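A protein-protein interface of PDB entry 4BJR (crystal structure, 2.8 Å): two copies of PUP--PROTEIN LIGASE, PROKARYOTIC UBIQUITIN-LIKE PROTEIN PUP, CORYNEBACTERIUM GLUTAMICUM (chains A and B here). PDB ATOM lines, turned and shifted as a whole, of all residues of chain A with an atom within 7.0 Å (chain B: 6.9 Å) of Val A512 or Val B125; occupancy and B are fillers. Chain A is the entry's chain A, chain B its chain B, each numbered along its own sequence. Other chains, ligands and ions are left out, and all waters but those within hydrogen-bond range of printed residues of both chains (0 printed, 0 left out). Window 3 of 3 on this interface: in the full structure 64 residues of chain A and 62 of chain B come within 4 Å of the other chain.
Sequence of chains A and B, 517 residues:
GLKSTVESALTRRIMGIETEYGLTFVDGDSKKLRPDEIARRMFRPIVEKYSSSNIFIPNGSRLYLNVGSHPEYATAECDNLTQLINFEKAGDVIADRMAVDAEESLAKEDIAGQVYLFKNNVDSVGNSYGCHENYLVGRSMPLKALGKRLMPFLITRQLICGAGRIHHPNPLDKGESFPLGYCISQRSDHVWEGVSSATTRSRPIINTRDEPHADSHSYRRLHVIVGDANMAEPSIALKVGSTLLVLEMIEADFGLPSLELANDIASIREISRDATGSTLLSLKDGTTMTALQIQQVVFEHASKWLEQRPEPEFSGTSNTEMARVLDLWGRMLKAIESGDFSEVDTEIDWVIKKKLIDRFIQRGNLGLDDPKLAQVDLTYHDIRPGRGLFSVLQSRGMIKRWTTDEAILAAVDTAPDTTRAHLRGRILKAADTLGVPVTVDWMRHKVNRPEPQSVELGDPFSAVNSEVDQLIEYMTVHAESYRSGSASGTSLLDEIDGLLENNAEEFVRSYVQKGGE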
ATOM      1  N   PHE A 507     -30.202   6.364 -24.284  1.00  0.00           N
ATOM      2  CA  PHE A 507     -29.851   6.719 -25.648  1.00  0.00           C
ATOM      3  C   PHE A 507     -30.425   8.066 -26.044  1.00  0.00           C
ATOM      4  O   PHE A 507     -29.712   8.925 -26.549  1.00  0.00           O
ATOM      5  CB  PHE A 507     -30.337   5.643 -26.611  1.00  0.00           C
ATOM      6  CG  PHE A 507     -29.974   5.891 -28.041  1.00  0.00           C
ATOM      7  CD1 PHE A 507     -28.686   5.727 -28.480  1.00  0.00           C
ATOM      8  CD2 PHE A 507     -30.931   6.264 -28.953  1.00  0.00           C
ATOM      9  CE1 PHE A 507     -28.363   5.949 -29.790  1.00  0.00           C
ATOM     10  CE2 PHE A 507     -30.605   6.481 -30.261  1.00  0.00           C
ATOM     11  CZ  PHE A 507     -29.322   6.325 -30.675  1.00  0.00           C
ATOM     12  N   VAL A 508     -31.711   8.258 -25.790  1.00  0.00           N
ATOM     13  CA  VAL A 508     -32.343   9.530 -26.092  1.00  0.00           C
ATOM     14  C   VAL A 508     -31.831  10.636 -25.174  1.00  0.00           C
ATOM     15  O   VAL A 508     -31.592  11.744 -25.632  1.00  0.00           O
ATOM     16  CB  VAL A 508     -33.881   9.426 -26.031  1.00  0.00           C
ATOM     17  CG1 VAL A 508     -34.317   8.622 -24.849  1.00  0.00           C
ATOM     18  CG2 VAL A 508     -34.513  10.790 -26.006  1.00  0.00           C
ATOM     19  N   ARG A 509     -31.645  10.349 -23.891  1.00  0.00           N
ATOM     20  CA  ARG A 509     -31.168  11.386 -22.979  1.00  0.00           C
ATOM     21  C   ARG A 509     -29.821  11.904 -23.411  1.00  0.00           C
ATOM     22  O   ARG A 509     -29.545  13.094 -23.351  1.00  0.00           O
ATOM     23  CB  ARG A 509     -31.035  10.866 -21.551  1.00  0.00           C
ATOM     24  CG  ARG A 509     -32.306  10.832 -20.742  1.00  0.00           C
ATOM     25  CD  ARG A 509     -32.019  11.007 -19.255  1.00  0.00           C
ATOM     26  NE  ARG A 509     -30.936  10.160 -18.763  1.00  0.00           N
ATOM     27  CZ  ARG A 509     -29.698  10.589 -18.551  1.00  0.00           C
ATOM     28  NH1 ARG A 509     -29.390  11.852 -18.797  1.00  0.00           N
ATOM     29  NH2 ARG A 509     -28.771   9.760 -18.100  1.00  0.00           N
ATOM     30  N   SER A 510     -28.981  10.979 -23.844  1.00  0.00           N
ATOM     31  CA  SER A 510     -27.626  11.293 -24.244  1.00  0.00           C
ATOM     32  C   SER A 510     -27.591  12.212 -25.440  1.00  0.00           C
ATOM     33  O   SER A 510     -26.732  13.073 -25.530  1.00  0.00           O
ATOM     34  CB  SER A 510     -26.868  10.015 -24.550  1.00  0.00           C
ATOM     35  OG  SER A 510     -27.694   9.125 -25.272  1.00  0.00           O
ATOM     36  N   TYR A 511     -28.529  12.039 -26.361  1.00  0.00           N
ATOM     37  CA  TYR A 511     -28.486  12.813 -27.590  1.00  0.00           C
ATOM     38  C   TYR A 511     -28.733  14.285 -27.328  1.00  0.00           C
ATOM     39  O   TYR A 511     -29.805  14.684 -26.891  1.00  0.00           O
ATOM     40  CB  TYR A 511     -29.509  12.273 -28.576  1.00  0.00           C
ATOM     41  CG  TYR A 511     -29.493  12.963 -29.910  1.00  0.00           C
ATOM     42  CD1 TYR A 511     -28.354  12.985 -30.686  1.00  0.00           C
ATOM     43  CD2 TYR A 511     -30.625  13.575 -30.399  1.00  0.00           C
ATOM     44  CE1 TYR A 511     -28.343  13.613 -31.900  1.00  0.00           C
ATOM     45  CE2 TYR A 511     -30.621  14.199 -31.610  1.00  0.00           C
ATOM     46  CZ  TYR A 511     -29.481  14.219 -32.355  1.00  0.00           C
ATOM     47  OH  TYR A 511     -29.490  14.850 -33.566  1.00  0.00           O
ATOM     48  N   VAL A 512     -27.733  15.088 -27.671  1.00  0.00           N
ATOM     49  CA  VAL A 512     -27.745  16.528 -27.471  1.00  0.00           C
ATOM     50  C   VAL A 512     -27.051  17.207 -28.640  1.00  0.00           C
ATOM     51  O   VAL A 512     -26.029  16.736 -29.122  1.00  0.00           O
ATOM     52  CB  VAL A 512     -27.038  16.925 -26.154  1.00  0.00           C
ATOM     53  CG1 VAL A 512     -27.001  18.418 -25.981  1.00  0.00           C
ATOM     54  CG2 VAL A 512     -27.712  16.291 -24.970  1.00  0.00           C
ATOM     55  N   GLN A 513     -27.607  18.331 -29.071  1.00  0.00           N
ATOM     56  CA  GLN A 513     -27.122  19.057 -30.233  1.00  0.00           C
ATOM     57  C   GLN A 513     -27.255  20.550 -30.008  1.00  0.00           C
ATOM     58  O   GLN A 513     -28.038  20.997 -29.181  1.00  0.00           O
ATOM     59  CB  GLN A 513     -27.884  18.644 -31.493  1.00  0.00           C
ATOM     60  CG  GLN A 513     -27.676  17.208 -31.944  1.00  0.00           C
ATOM     61  CD  GLN A 513     -26.418  17.017 -32.753  1.00  0.00           C
ATOM     62  OE1 GLN A 513     -26.142  17.773 -33.676  1.00  0.00           O
ATOM     63  NE2 GLN A 513     -25.646  16.003 -32.411  1.00  0.00           N
ATOM     64  N   LYS A 514     -26.463  21.308 -30.745  1.00  0.00           N
ATOM     65  CA  LYS A 514     -26.509  22.761 -30.746  1.00  0.00           C
ATOM     66  C   LYS A 514     -27.404  23.247 -31.877  1.00  0.00           C
ATOM     67  O   LYS A 514     -27.521  22.573 -32.875  1.00  0.00           O
ATOM     68  CB  LYS A 514     -25.101  23.315 -30.902  1.00  0.00           C
ATOM     69  CG  LYS A 514     -24.247  23.081 -29.688  1.00  0.00           C
ATOM     70  CD  LYS A 514     -22.839  22.667 -30.066  1.00  0.00           C
ATOM     71  CE  LYS A 514     -22.033  23.832 -30.606  1.00  0.00           C
ATOM     72  NZ  LYS A 514     -20.659  23.421 -31.016  1.00  0.00           N
ATOM     73  N   LEU B  23     -25.902  14.781 -35.587  1.00  0.00           N
ATOM     74  CA  LEU B  23     -24.763  13.886 -35.545  1.00  0.00           C
ATOM     75  C   LEU B  23     -24.369  13.494 -34.141  1.00  0.00           C
ATOM     76  O   LEU B  23     -24.214  14.347 -33.278  1.00  0.00           O
ATOM     77  CB  LEU B  23     -23.576  14.533 -36.240  1.00  0.00           C
ATOM     78  CG  LEU B  23     -22.241  13.808 -36.184  1.00  0.00           C
ATOM     79  CD1 LEU B  23     -22.326  12.521 -36.943  1.00  0.00           C
ATOM     80  CD2 LEU B  23     -21.190  14.689 -36.778  1.00  0.00           C
ATOM     81  N   THR B  24     -24.200  12.203 -33.903  1.00  0.00           N
ATOM     82  CA  THR B  24     -23.669  11.780 -32.618  1.00  0.00           C
ATOM     83  C   THR B  24     -22.842  10.507 -32.733  1.00  0.00           C
ATOM     84  O   THR B  24     -23.001   9.736 -33.663  1.00  0.00           O
ATOM     85  CB  THR B  24     -24.788  11.582 -31.588  1.00  0.00           C
ATOM     86  OG1 THR B  24     -24.228  11.518 -30.274  1.00  0.00           O
ATOM     87  CG2 THR B  24     -25.563  10.331 -31.874  1.00  0.00           C
ATOM     88  N   LYS B  31     -22.422   8.547 -24.603  1.00  0.00           N
ATOM     89  CA  LYS B  31     -21.986   9.150 -25.848  1.00  0.00           C
ATOM     90  C   LYS B  31     -20.467   9.189 -25.866  1.00  0.00           C
ATOM     91  O   LYS B  31     -19.826   9.769 -24.998  1.00  0.00           O
ATOM     92  CB  LYS B  31     -22.587  10.542 -26.049  1.00  0.00           C
ATOM     93  CG  LYS B  31     -22.239  11.559 -24.998  1.00  0.00           C
ATOM     94  CD  LYS B  31     -22.408  12.980 -25.521  1.00  0.00           C
ATOM     95  CE  LYS B  31     -23.793  13.210 -26.073  1.00  0.00           C
ATOM     96  NZ  LYS B  31     -23.875  14.414 -26.937  1.00  0.00           N
ATOM     97  N   PRO B  35     -20.002  16.155 -30.450  1.00  0.00           N
ATOM     98  CA  PRO B  35     -20.443  16.336 -31.826  1.00  0.00           C
ATOM     99  C   PRO B  35     -19.447  17.106 -32.670  1.00  0.00           C
ATOM    100  O   PRO B  35     -19.266  16.761 -33.822  1.00  0.00           O
ATOM    101  CB  PRO B  35     -21.742  17.110 -31.664  1.00  0.00           C
ATOM    102  CG  PRO B  35     -22.267  16.657 -30.381  1.00  0.00           C
ATOM    103  CD  PRO B  35     -21.087  16.420 -29.495  1.00  0.00           C
ATOM    104  N   VAL B 122     -34.874  18.152 -34.367  1.00  0.00           N
ATOM    105  CA  VAL B 122     -34.773  18.393 -32.926  1.00  0.00           C
ATOM    106  C   VAL B 122     -33.975  17.367 -32.145  1.00  0.00           C
ATOM    107  O   VAL B 122     -33.697  16.278 -32.621  1.00  0.00           O
ATOM    108  CB  VAL B 122     -36.143  18.443 -32.259  1.00  0.00           C
ATOM    109  CG1 VAL B 122     -36.901  19.656 -32.710  1.00  0.00           C
ATOM    110  CG2 VAL B 122     -36.909  17.212 -32.588  1.00  0.00           C
ATOM    111  N   ASP B 123     -33.636  17.743 -30.921  1.00  0.00           N
ATOM    112  CA  ASP B 123     -32.942  16.882 -29.984  1.00  0.00           C
ATOM    113  C   ASP B 123     -33.702  16.828 -28.670  1.00  0.00           C
ATOM    114  O   ASP B 123     -34.619  17.607 -28.454  1.00  0.00           O
ATOM    115  CB  ASP B 123     -31.512  17.373 -29.775  1.00  0.00           C
ATOM    116  CG  ASP B 123     -31.422  18.548 -28.836  1.00  0.00           C
ATOM    117  OD1 ASP B 123     -32.415  19.271 -28.661  1.00  0.00           O
ATOM    118  OD2 ASP B 123     -30.327  18.780 -28.294  1.00  0.00           O
ATOM    119  N   SER B 124     -33.327  15.897 -27.806  1.00  0.00           N
ATOM    120  CA  SER B 124     -33.985  15.698 -26.518  1.00  0.00           C
ATOM    121  C   SER B 124     -34.068  16.957 -25.670  1.00  0.00           C
ATOM    122  O   SER B 124     -35.055  17.185 -24.986  1.00  0.00           O
ATOM    123  CB  SER B 124     -33.258  14.614 -25.739  1.00  0.00           C
ATOM    124  OG  SER B 124     -33.075  13.471 -26.544  1.00  0.00           O
ATOM    125  N   VAL B 125     -33.018  17.763 -25.711  1.00  0.00           N
ATOM    126  CA  VAL B 125     -32.992  19.040 -25.017  1.00  0.00           C
ATOM    127  C   VAL B 125     -33.974  20.046 -25.598  1.00  0.00           C
ATOM    128  O   VAL B 125     -34.525  20.869 -24.879  1.00  0.00           O
ATOM    129  CB  VAL B 125     -31.594  19.642 -25.065  1.00  0.00           C
ATOM    130  CG1 VAL B 125     -31.514  20.873 -24.203  1.00  0.00           C
ATOM    131  CG2 VAL B 125     -30.590  18.624 -24.610  1.00  0.00           C
ATOM    132  N   GLY B 126     -34.212  19.965 -26.901  1.00  0.00           N
ATOM    133  CA  GLY B 126     -35.046  20.945 -27.562  1.00  0.00           C
ATOM    134  C   GLY B 126     -34.358  21.995 -28.417  1.00  0.00           C
ATOM    135  O   GLY B 126     -34.966  23.002 -28.755  1.00  0.00           O
ATOM    136  N   ASN B 127     -33.088  21.792 -28.739  1.00  0.00           N
ATOM    137  CA  ASN B 127     -32.433  22.610 -29.750  1.00  0.00           C
ATOM    138  C   ASN B 127     -32.907  22.215 -31.131  1.00  0.00           C
ATOM    139  O   ASN B 127     -33.278  21.071 -31.347  1.00  0.00           O
ATOM    140  CB  ASN B 127     -30.923  22.486 -29.671  1.00  0.00           C
ATOM    141  CG  ASN B 127     -30.411  22.616 -28.277  1.00  0.00           C
ATOM    142  OD1 ASN B 127     -30.336  23.709 -27.735  1.00  0.00           O
ATOM    143  ND2 ASN B 127     -30.032  21.500 -27.687  1.00  0.00           N
ATOM    144  N   TYR B 129     -32.425  22.319 -35.491  1.00  0.00           N
ATOM    145  CA  TYR B 129     -31.722  22.533 -36.738  1.00  0.00           C
ATOM    146  C   TYR B 129     -32.677  22.261 -37.894  1.00  0.00           C
ATOM    147  O   TYR B 129     -33.441  21.310 -37.850  1.00  0.00           O
ATOM    148  CB  TYR B 129     -30.485  21.638 -36.814  1.00  0.00           C
ATOM    149  CG  TYR B 129     -30.642  20.296 -36.136  1.00  0.00           C
ATOM    150  CD1 TYR B 129     -30.484  20.159 -34.768  1.00  0.00           C
ATOM    151  CD2 TYR B 129     -30.963  19.176 -36.860  1.00  0.00           C
ATOM    152  CE1 TYR B 129     -30.637  18.951 -34.160  1.00  0.00           C
ATOM    153  CE2 TYR B 129     -31.116  17.969 -36.252  1.00  0.00           C
ATOM    154  CZ  TYR B 129     -30.955  17.859 -34.909  1.00  0.00           C
ATOM    155  OH  TYR B 129     -31.110  16.634 -34.320  1.00  0.00           O
ATOM    156  N   HIS B 190     -40.110  25.901 -32.448  1.00  0.00           N
ATOM    157  CA  HIS B 190     -38.846  26.595 -32.609  1.00  0.00           C
ATOM    158  C   HIS B 190     -38.919  27.782 -33.553  1.00  0.00           C
ATOM    159  O   HIS B 190     -38.288  28.805 -33.318  1.00  0.00           O
ATOM    160  CB  HIS B 190     -37.793  25.602 -33.068  1.00  0.00           C
ATOM    161  CG  HIS B 190     -37.588  24.487 -32.097  1.00  0.00           C
ATOM    162  ND1 HIS B 190     -38.341  23.335 -32.117  1.00  0.00           N
ATOM    163  CD2 HIS B 190     -36.769  24.380 -31.023  1.00  0.00           C
ATOM    164  CE1 HIS B 190     -37.965  22.546 -31.127  1.00  0.00           C
ATOM    165  NE2 HIS B 190     -37.013  23.160 -30.448  1.00  0.00           N
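O of Gln A513 sits at hydrogen-bond distance from ND2 of Asn B127 (2.5 Å). O of Ser A510 lies close to NZ of Lys B31 (3.5 Å). N of Leu B23 lies close to NE2 of Gln A513. N of Gln A513 lies within hydrogen-bond range of OD2 of Asp B123, at 2.9 Å. The backbone carbonyl oxygen (O) of Val A508 is in hydrogen-bond range of the side-chain hydroxyl (OG) of Ser B124, at 2.5 Å. The side-chain hydroxyl (OH) of Tyr A511 lies within hydrogen-bond range of the side-chain hydroxyl (OH) of Tyr B129 (2.5 Å).
OH of Tyr B129 is in hydrogen-bond range of O of Val B122 (3.1 Å). N of Asn B127 lies within hydrogen-bond range of OD1 of Asp B123 (2.6 Å). OD1 of Asp B123 sits at hydrogen-bond distance from N of Gly B126. The backbone NH (N) of Val B125 lies close to the side-chain carboxylate (OD1) of Asp B123, 3.4 Å away.
Thr B24 touches Tyr A511 (CB to CD1, 3.9 Å). Tyr A511 touches Val B122 (CE2 to O, 3.8 Å). Tyr A511 touches Asp B123. Ser B124 touches Tyr A511. Val A512 touches Lys B31 (O to NZ, 3.8 Å). Val A512 touches Pro B35 (O to CG, 3.97 Å). Asp B123 touches Val A512 (OD2 to CA, 3.5 Å). CG2 of Val A512 touches CG2 of Val B125 (3.7 Å). NE2 of Gln A513 touches CG of Pro B35, at 3.996 Å. Tyr B129 touches Gln A513.
Val A512 touches just these residues of chain B: Lys B31, Pro B35, Asp B123 and Val B125. Val B125 touches just one residue of chain A: Val A512 (3.7 Å). Printed residues of chain B within 4 Å of Ser A510: Lys B31 (3.0 Å). Printed residues of chain A within 4 Å of Asp B123: Tyr A511 (3.8 Å), Val A512 (3.5 Å) and Gln A513 (2.9 Å). His B190 touches none of the printed residues of chain A. Gly B126 touches none of the printed residues of chain A.
Printed residues of chain A that touch a printed residue of chain B: Val A508, Ser A510, Tyr A511, Val A512 and Gln A513. Among the printed residues, 16 pairs touch across the chains. Among the printed residues, no Asp or Glu carboxylate lies within 4 Å of a Lys or Arg side-chain nitrogen of the other chain.
No position is printed for both chains.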
